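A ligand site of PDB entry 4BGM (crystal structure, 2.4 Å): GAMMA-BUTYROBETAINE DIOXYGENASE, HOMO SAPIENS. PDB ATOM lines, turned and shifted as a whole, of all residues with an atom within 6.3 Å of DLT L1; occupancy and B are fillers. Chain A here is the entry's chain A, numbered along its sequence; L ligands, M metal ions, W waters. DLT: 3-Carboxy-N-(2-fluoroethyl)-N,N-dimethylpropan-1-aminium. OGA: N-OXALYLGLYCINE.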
ATOM      1  N   THR A 175     -18.143 -20.019   8.929  1.00  0.00           N
ATOM      2  CA  THR A 175     -18.925 -20.651   7.858  1.00  0.00           C
ATOM      3  C   THR A 175     -19.339 -22.021   8.292  1.00  0.00           C
ATOM      4  O   THR A 175     -19.070 -22.426   9.415  1.00  0.00           O
ATOM      5  CB  THR A 175     -18.187 -20.692   6.511  1.00  0.00           C
ATOM      6  OG1 THR A 175     -17.108 -21.659   6.542  1.00  0.00           O
ATOM      7  CG2 THR A 175     -17.634 -19.321   6.173  1.00  0.00           C
ATOM      8  N   TYR A 177     -18.119 -24.640   7.396  1.00  0.00           N
ATOM      9  CA  TYR A 177     -16.944 -25.494   7.511  1.00  0.00           C
ATOM     10  C   TYR A 177     -16.152 -25.186   8.757  1.00  0.00           C
ATOM     11  O   TYR A 177     -15.061 -25.702   8.913  1.00  0.00           O
ATOM     12  CB  TYR A 177     -16.092 -25.357   6.250  1.00  0.00           C
ATOM     13  CG  TYR A 177     -16.734 -26.021   5.050  1.00  0.00           C
ATOM     14  CD1 TYR A 177     -16.575 -27.389   4.817  1.00  0.00           C
ATOM     15  CD2 TYR A 177     -17.513 -25.285   4.131  1.00  0.00           C
ATOM     16  CE1 TYR A 177     -17.161 -28.004   3.728  1.00  0.00           C
ATOM     17  CE2 TYR A 177     -18.106 -25.900   3.034  1.00  0.00           C
ATOM     18  CZ  TYR A 177     -17.913 -27.254   2.827  1.00  0.00           C
ATOM     19  OH  TYR A 177     -18.493 -27.883   1.744  1.00  0.00           O
ATOM     20  N   TRP A 181     -10.640 -24.570   9.455  1.00  0.00           N
ATOM     21  CA  TRP A 181     -10.915 -25.837   8.826  1.00  0.00           C
ATOM     22  C   TRP A 181      -9.625 -26.456   8.360  1.00  0.00           C
ATOM     23  O   TRP A 181      -8.641 -25.748   8.134  1.00  0.00           O
ATOM     24  CB  TRP A 181     -11.881 -25.701   7.642  1.00  0.00           C
ATOM     25  CG  TRP A 181     -11.894 -24.385   6.996  1.00  0.00           C
ATOM     26  CD1 TRP A 181     -12.715 -23.347   7.288  1.00  0.00           C
ATOM     27  CD2 TRP A 181     -11.052 -23.947   5.919  1.00  0.00           C
ATOM     28  NE1 TRP A 181     -12.437 -22.282   6.468  1.00  0.00           N
ATOM     29  CE2 TRP A 181     -11.415 -22.624   5.617  1.00  0.00           C
ATOM     30  CE3 TRP A 181     -10.021 -24.543   5.173  1.00  0.00           C
ATOM     31  CZ2 TRP A 181     -10.804 -21.905   4.610  1.00  0.00           C
ATOM     32  CZ3 TRP A 181      -9.411 -23.818   4.179  1.00  0.00           C
ATOM     33  CH2 TRP A 181      -9.812 -22.522   3.904  1.00  0.00           C
ATOM     34  N   VAL A 183      -7.503 -28.683   5.719  1.00  0.00           N
ATOM     35  CA  VAL A 183      -7.416 -29.133   4.320  1.00  0.00           C
ATOM     36  C   VAL A 183      -6.455 -30.306   4.253  1.00  0.00           C
ATOM     37  O   VAL A 183      -5.245 -30.141   4.344  1.00  0.00           O
ATOM     38  CB  VAL A 183      -6.940 -28.024   3.369  1.00  0.00           C
ATOM     39  CG1 VAL A 183      -6.874 -28.507   1.921  1.00  0.00           C
ATOM     40  CG2 VAL A 183      -7.873 -26.839   3.477  1.00  0.00           C
ATOM     41  N   ASN A 190     -16.640 -34.426   2.263  1.00  0.00           N
ATOM     42  CA  ASN A 190     -17.756 -33.537   1.933  1.00  0.00           C
ATOM     43  C   ASN A 190     -17.378 -32.437   0.929  1.00  0.00           C
ATOM     44  O   ASN A 190     -18.198 -31.558   0.642  1.00  0.00           O
ATOM     45  CB  ASN A 190     -18.412 -32.933   3.211  1.00  0.00           C
ATOM     46  CG  ASN A 190     -17.532 -31.901   3.945  1.00  0.00           C
ATOM     47  OD1 ASN A 190     -16.488 -31.473   3.450  1.00  0.00           O
ATOM     48  ND2 ASN A 190     -17.974 -31.515   5.155  1.00  0.00           N
ATOM     49  N   ASN A 191     -16.154 -32.451   0.418  1.00  0.00           N
ATOM     50  CA  ASN A 191     -15.677 -31.340  -0.410  1.00  0.00           C
ATOM     51  C   ASN A 191     -14.414 -31.730  -1.179  1.00  0.00           C
ATOM     52  O   ASN A 191     -13.530 -32.355  -0.616  1.00  0.00           O
ATOM     53  CB  ASN A 191     -15.418 -30.125   0.489  1.00  0.00           C
ATOM     54  CG  ASN A 191     -15.304 -28.806  -0.285  1.00  0.00           C
ATOM     55  OD1 ASN A 191     -14.316 -28.565  -0.947  1.00  0.00           O
ATOM     56  ND2 ASN A 191     -16.298 -27.956  -0.162  1.00  0.00           N
ATOM     57  N   VAL A 192     -14.317 -31.350  -2.459  1.00  0.00           N
ATOM     58  CA  VAL A 192     -13.172 -31.786  -3.281  1.00  0.00           C
ATOM     59  C   VAL A 192     -11.834 -31.280  -2.758  1.00  0.00           C
ATOM     60  O   VAL A 192     -10.783 -31.864  -3.060  1.00  0.00           O
ATOM     61  CB  VAL A 192     -13.280 -31.400  -4.770  1.00  0.00           C
ATOM     62  CG1 VAL A 192     -14.484 -32.069  -5.410  1.00  0.00           C
ATOM     63  CG2 VAL A 192     -13.361 -29.890  -4.946  1.00  0.00           C
ATOM     64  N   ALA A 193     -11.867 -30.195  -1.987  1.00  0.00           N
ATOM     65  CA  ALA A 193     -10.650 -29.697  -1.340  1.00  0.00           C
ATOM     66  C   ALA A 193     -10.049 -30.735  -0.392  1.00  0.00           C
ATOM     67  O   ALA A 193      -8.839 -30.770  -0.175  1.00  0.00           O
ATOM     68  CB  ALA A 193     -10.954 -28.415  -0.609  1.00  0.00           C
ATOM     69  N   TYR A 194     -10.915 -31.577   0.175  1.00  0.00           N
ATOM     70  CA  TYR A 194     -10.528 -32.609   1.106  1.00  0.00           C
ATOM     71  C   TYR A 194     -10.238 -34.003   0.417  1.00  0.00           C
ATOM     72  O   TYR A 194     -10.682 -35.064   0.876  1.00  0.00           O
ATOM     73  CB  TYR A 194     -11.621 -32.731   2.184  1.00  0.00           C
ATOM     74  CG  TYR A 194     -11.962 -31.418   2.932  1.00  0.00           C
ATOM     75  CD1 TYR A 194     -11.020 -30.353   3.064  1.00  0.00           C
ATOM     76  CD2 TYR A 194     -13.208 -31.263   3.566  1.00  0.00           C
ATOM     77  CE1 TYR A 194     -11.338 -29.190   3.763  1.00  0.00           C
ATOM     78  CE2 TYR A 194     -13.508 -30.107   4.276  1.00  0.00           C
ATOM     79  CZ  TYR A 194     -12.574 -29.088   4.375  1.00  0.00           C
ATOM     80  OH  TYR A 194     -12.900 -27.969   5.077  1.00  0.00           O
ATOM     81  N   HIS A 202     -10.082 -21.340  -8.797  1.00  0.00           N
ATOM     82  CA  HIS A 202     -11.398 -21.043  -8.267  1.00  0.00           C
ATOM     83  C   HIS A 202     -11.297 -19.933  -7.232  1.00  0.00           C
ATOM     84  O   HIS A 202     -10.184 -19.610  -6.766  1.00  0.00           O
ATOM     85  CB  HIS A 202     -12.010 -22.297  -7.595  1.00  0.00           C
ATOM     86  CG  HIS A 202     -11.229 -22.810  -6.419  1.00  0.00           C
ATOM     87  ND1 HIS A 202     -10.041 -23.479  -6.564  1.00  0.00           N
ATOM     88  CD2 HIS A 202     -11.464 -22.750  -5.091  1.00  0.00           C
ATOM     89  CE1 HIS A 202      -9.575 -23.819  -5.372  1.00  0.00           C
ATOM     90  NE2 HIS A 202     -10.418 -23.376  -4.461  1.00  0.00           N
ATOM     91  N   THR A 203     -12.439 -19.377  -6.866  1.00  0.00           N
ATOM     92  CA  THR A 203     -12.554 -18.595  -5.653  1.00  0.00           C
ATOM     93  C   THR A 203     -13.267 -19.488  -4.703  1.00  0.00           C
ATOM     94  O   THR A 203     -13.923 -20.399  -5.136  1.00  0.00           O
ATOM     95  CB  THR A 203     -13.339 -17.273  -5.857  1.00  0.00           C
ATOM     96  OG1 THR A 203     -14.690 -17.513  -6.281  1.00  0.00           O
ATOM     97  CG2 THR A 203     -12.640 -16.417  -6.883  1.00  0.00           C
ATOM     98  N   ASP A 204     -13.142 -19.231  -3.406  1.00  0.00           N
ATOM     99  CA  ASP A 204     -13.780 -20.047  -2.372  1.00  0.00           C
ATOM    100  C   ASP A 204     -15.141 -19.499  -2.031  1.00  0.00           C
ATOM    101  O   ASP A 204     -15.336 -18.288  -1.954  1.00  0.00           O
ATOM    102  CB  ASP A 204     -12.938 -20.080  -1.105  1.00  0.00           C
ATOM    103  CG  ASP A 204     -12.006 -21.291  -1.039  1.00  0.00           C
ATOM    104  OD1 ASP A 204     -11.553 -21.804  -2.116  1.00  0.00           O
ATOM    105  OD2 ASP A 204     -11.699 -21.668   0.118  1.00  0.00           O
ATOM    106  N   TYR A 205     -16.073 -20.434  -1.842  1.00  0.00           N
ATOM    107  CA  TYR A 205     -17.429 -20.227  -1.374  1.00  0.00           C
ATOM    108  C   TYR A 205     -18.363 -19.361  -2.223  1.00  0.00           C
ATOM    109  O   TYR A 205     -19.160 -18.598  -1.677  1.00  0.00           O
ATOM    110  CB  TYR A 205     -17.411 -19.774   0.074  1.00  0.00           C
ATOM    111  CG  TYR A 205     -18.074 -20.705   1.096  1.00  0.00           C
ATOM    112  CD1 TYR A 205     -19.289 -21.335   0.825  1.00  0.00           C
ATOM    113  CD2 TYR A 205     -17.501 -20.922   2.352  1.00  0.00           C
ATOM    114  CE1 TYR A 205     -19.892 -22.167   1.758  1.00  0.00           C
ATOM    115  CE2 TYR A 205     -18.105 -21.740   3.287  1.00  0.00           C
ATOM    116  CZ  TYR A 205     -19.309 -22.360   2.997  1.00  0.00           C
ATOM    117  OH  TYR A 205     -19.943 -23.167   3.941  1.00  0.00           O
ATOM    118  N   PRO A 206     -18.346 -19.516  -3.570  1.00  0.00           N
ATOM    119  CA  PRO A 206     -19.397 -18.846  -4.343  1.00  0.00           C
ATOM    120  C   PRO A 206     -20.820 -19.342  -4.021  1.00  0.00           C
ATOM    121  O   PRO A 206     -21.805 -18.644  -4.332  1.00  0.00           O
ATOM    122  CB  PRO A 206     -19.024 -19.178  -5.772  1.00  0.00           C
ATOM    123  CG  PRO A 206     -18.289 -20.472  -5.666  1.00  0.00           C
ATOM    124  CD  PRO A 206     -17.427 -20.248  -4.451  1.00  0.00           C
ATOM    125  N   ALA A 207     -20.929 -20.520  -3.416  1.00  0.00           N
ATOM    126  CA  ALA A 207     -22.235 -21.004  -2.918  1.00  0.00           C
ATOM    127  C   ALA A 207     -22.881 -20.042  -1.915  1.00  0.00           C
ATOM    128  O   ALA A 207     -24.057 -20.155  -1.656  1.00  0.00           O
ATOM    129  CB  ALA A 207     -22.102 -22.380  -2.290  1.00  0.00           C
ATOM    130  N   GLN A 215      -8.856 -14.839   2.527  1.00  0.00           N
ATOM    131  CA  GLN A 215      -8.615 -16.227   2.878  1.00  0.00           C
ATOM    132  C   GLN A 215      -7.250 -16.349   3.486  1.00  0.00           C
ATOM    133  O   GLN A 215      -6.297 -15.713   3.043  1.00  0.00           O
ATOM    134  CB  GLN A 215      -8.744 -17.148   1.650  1.00  0.00           C
ATOM    135  CG  GLN A 215      -8.536 -18.634   1.958  1.00  0.00           C
ATOM    136  CD  GLN A 215      -8.872 -19.562   0.783  1.00  0.00           C
ATOM    137  OE1 GLN A 215      -8.371 -20.698   0.695  1.00  0.00           O
ATOM    138  NE2 GLN A 215      -9.695 -19.082  -0.117  1.00  0.00           N
ATOM    139  N   LEU A 217      -4.510 -19.418   4.592  1.00  0.00           N
ATOM    140  CA  LEU A 217      -4.144 -20.824   4.467  1.00  0.00           C
ATOM    141  C   LEU A 217      -2.754 -20.970   5.055  1.00  0.00           C
ATOM    142  O   LEU A 217      -1.812 -20.274   4.648  1.00  0.00           O
ATOM    143  CB  LEU A 217      -4.077 -21.262   3.007  1.00  0.00           C
ATOM    144  CG  LEU A 217      -5.318 -21.759   2.266  1.00  0.00           C
ATOM    145  CD1 LEU A 217      -4.860 -22.358   0.935  1.00  0.00           C
ATOM    146  CD2 LEU A 217      -6.097 -22.795   3.046  1.00  0.00           C
ATOM    147  N   ASP A 261     -24.182 -26.306  -2.399  1.00  0.00           N
ATOM    148  CA  ASP A 261     -23.350 -27.042  -1.432  1.00  0.00           C
ATOM    149  C   ASP A 261     -24.292 -27.681  -0.415  1.00  0.00           C
ATOM    150  O   ASP A 261     -24.957 -26.957   0.330  1.00  0.00           O
ATOM    151  CB  ASP A 261     -22.347 -26.109  -0.744  1.00  0.00           C
ATOM    152  CG  ASP A 261     -21.158 -26.845  -0.124  1.00  0.00           C
ATOM    153  OD1 ASP A 261     -20.844 -27.999  -0.509  1.00  0.00           O
ATOM    154  OD2 ASP A 261     -20.532 -26.241   0.762  1.00  0.00           O
ATOM    155  N   ASN A 292     -16.231 -21.262  -8.512  1.00  0.00           N
ATOM    156  CA  ASN A 292     -15.605 -22.534  -8.164  1.00  0.00           C
ATOM    157  C   ASN A 292     -16.297 -23.616  -9.025  1.00  0.00           C
ATOM    158  O   ASN A 292     -17.495 -23.766  -8.975  1.00  0.00           O
ATOM    159  CB  ASN A 292     -15.715 -22.796  -6.658  1.00  0.00           C
ATOM    160  CG  ASN A 292     -15.146 -24.143  -6.248  1.00  0.00           C
ATOM    161  OD1 ASN A 292     -14.888 -25.010  -7.087  1.00  0.00           O
ATOM    162  ND2 ASN A 292     -14.973 -24.346  -4.946  1.00  0.00           N
ATOM    163  N   ALA A 294     -16.179 -26.749  -8.856  1.00  0.00           N
ATOM    164  CA  ALA A 294     -16.662 -27.871  -8.062  1.00  0.00           C
ATOM    165  C   ALA A 294     -18.117 -27.659  -7.645  1.00  0.00           C
ATOM    166  O   ALA A 294     -18.925 -28.576  -7.731  1.00  0.00           O
ATOM    167  CB  ALA A 294     -15.782 -28.082  -6.831  1.00  0.00           C
ATOM    168  N   THR A 295     -18.430 -26.443  -7.232  1.00  0.00           N
ATOM    169  CA  THR A 295     -19.716 -26.143  -6.587  1.00  0.00           C
ATOM    170  C   THR A 295     -20.683 -25.464  -7.508  1.00  0.00           C
ATOM    171  O   THR A 295     -21.783 -25.131  -7.097  1.00  0.00           O
ATOM    172  CB  THR A 295     -19.518 -25.280  -5.301  1.00  0.00           C
ATOM    173  OG1 THR A 295     -19.029 -23.979  -5.632  1.00  0.00           O
ATOM    174  CG2 THR A 295     -18.528 -25.968  -4.335  1.00  0.00           C
ATOM    175  N   TYR A 366     -11.292 -17.686   7.021  1.00  0.00           N
ATOM    176  CA  TYR A 366     -11.726 -16.557   6.215  1.00  0.00           C
ATOM    177  C   TYR A 366     -11.942 -15.342   7.103  1.00  0.00           C
ATOM    178  O   TYR A 366     -12.077 -15.468   8.323  1.00  0.00           O
ATOM    179  CB  TYR A 366     -13.068 -16.872   5.570  1.00  0.00           C
ATOM    180  CG  TYR A 366     -13.082 -18.035   4.631  1.00  0.00           C
ATOM    181  CD1 TYR A 366     -12.231 -18.091   3.509  1.00  0.00           C
ATOM    182  CD2 TYR A 366     -13.964 -19.089   4.827  1.00  0.00           C
ATOM    183  CE1 TYR A 366     -12.281 -19.165   2.638  1.00  0.00           C
ATOM    184  CE2 TYR A 366     -14.026 -20.150   3.965  1.00  0.00           C
ATOM    185  CZ  TYR A 366     -13.199 -20.190   2.875  1.00  0.00           C
ATOM    186  OH  TYR A 366     -13.281 -21.285   2.051  1.00  0.00           O
HETATM  187  CAF DLT L   1     -13.833 -25.266   3.251  1.00  0.00           C
HETATM  188  CAE DLT L   1     -13.935 -23.857   3.816  1.00  0.00           C
HETATM  189  CAA DLT L   1     -11.883 -24.905   1.842  1.00  0.00           C
HETATM  190  CAH DLT L   1     -13.341 -26.777   1.527  1.00  0.00           C
HETATM  191  CAJ DLT L   1     -14.170 -24.572   0.977  1.00  0.00           C
HETATM  192  CAK DLT L   1     -13.880 -24.826  -0.512  1.00  0.00           C
HETATM  193  CAL DLT L   1     -14.484 -23.751  -1.406  1.00  0.00           C
HETATM  194  CAM DLT L   1     -15.883 -24.050  -1.836  1.00  0.00           C
HETATM  195  N3  DLT L   1     -13.290 -25.341   1.883  1.00  0.00           N
HETATM  196  OAC DLT L   1     -16.543 -25.025  -1.414  1.00  0.00           O
HETATM  197  F26 DLT L   1     -15.103 -23.271   3.409  1.00  0.00           F
HETATM  198  OAB DLT L   1     -16.361 -23.232  -2.637  1.00  0.00           O
HETATM  199  C1  OGA L   2      -9.202 -25.069  -0.932  1.00  0.00           C
HETATM  200  C2  OGA L   2      -7.938 -24.806  -1.596  1.00  0.00           C
HETATM  201  C4  OGA L   2      -5.611 -25.245  -1.844  1.00  0.00           C
HETATM  202  C5  OGA L   2      -4.590 -26.240  -1.400  1.00  0.00           C
HETATM  203  O1  OGA L   2     -10.202 -24.407  -1.259  1.00  0.00           O
HETATM  204  O2  OGA L   2      -9.228 -25.939  -0.013  1.00  0.00           O
HETATM  205  O2' OGA L   2      -7.830 -23.936  -2.451  1.00  0.00           O
HETATM  206  O3  OGA L   2      -3.429 -25.933  -1.675  1.00  0.00           O
HETATM  207  N1  OGA L   2      -6.888 -25.499  -1.207  1.00  0.00           N
HETATM  208  O4  OGA L   2      -4.916 -27.312  -0.817  1.00  0.00           O
HETATM  209 ZN    ZN M   1      -9.817 -22.891  -2.347  1.00  0.00          ZN
HETATM  210  O   HOH W   1     -19.137 -24.484  -1.040  1.00  0.00           O
HETATM  211  O   HOH W   2     -19.036 -22.635  -3.056  1.00  0.00           O
HETATM  212  O   HOH W   3     -14.581 -26.990  -3.478  1.00  0.00           O
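An oxygen (OAC) of DLT L1 lies within hydrogen-bond range of the side-chain amide nitrogen (ND2) of Asn 191 (3.2 Å). An oxygen (OAB) of DLT L1 lies within hydrogen-bond range of the backbone NH (N) of Tyr 205 (2.9 Å). The side-chain amide nitrogen (ND2) of Asn 292 lies within hydrogen-bond range of an oxygen (OAB) of DLT L1, 2.9 Å away.
OH of Tyr 366 lies close to F26 of DLT L1 (3.0 Å). Tyr 177 touches DLT L1 (CD2 to F26, 3.2 Å). CE2 of Trp 181 touches CAE of DLT L1, at 3.3 Å. Ala 193 touches DLT L1. Tyr 194 touches DLT L1 (OH to CAF, 3.4 Å). CG of Asp 204 touches CAL of DLT L1, at 3.5 Å. Pro 206 touches DLT L1 (CD to OAB, 3.7 Å). CG2 of Thr 295 touches OAC of DLT L1, at 3.7 Å. Hydrophobic or aromatic side chains within 4 Å of DLT L1: Tyr 177, Trp 181, Ala 193, Tyr 194, Tyr 205, Pro 206 and Tyr 366. 11 residues have an atom within 4 Å of DLT L1: Tyr 177, Trp 181, Asn 191, Ala 193, Tyr 194, Asp 204, Tyr 205, Pro 206, Asn 292, Thr 295 and Tyr 366.
Water W1 lies within hydrogen-bond range of OAC of DLT L1 (2.7 Å) and OD2 of Asp 261 (2.9 Å). Water W2 lies within hydrogen-bond range of OAB of DLT L1, N of Ala 207 and OG1 of Thr 295. Water W3 lies within hydrogen-bond range of OD1 of Asn 191 (3.0 Å), ND2 of Asn 292 (3.0 Å) and OAC of DLT L1 (3.5 Å).
OD1 of Asn 191 lies close to N of Ala 193 (3.1 Å). OH of Tyr 366 lies within hydrogen-bond range of OD2 of Asp 204, at 2.5 Å. N of Tyr 177 sits close to OG1 of Thr 175 (3.3 Å). The side-chain carboxylate (OD2) of Asp 204 sits at hydrogen-bond distance from the side-chain amide nitrogen (NE2) of Gln 215. The side-chain hydroxyl (OH) of Tyr 177 is in hydrogen-bond range of the side-chain carboxylate (OD2) of Asp 261, at 2.8 Å. The side-chain amide oxygen (OD1) of Asn 292 sits at hydrogen-bond distance from the backbone NH (N) of Ala 294, at 2.8 Å. The side-chain hydroxyl of Tyr 177 is in hydrogen-bond range of the side-chain amide nitrogen of Asn 191, at 2.9 Å.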
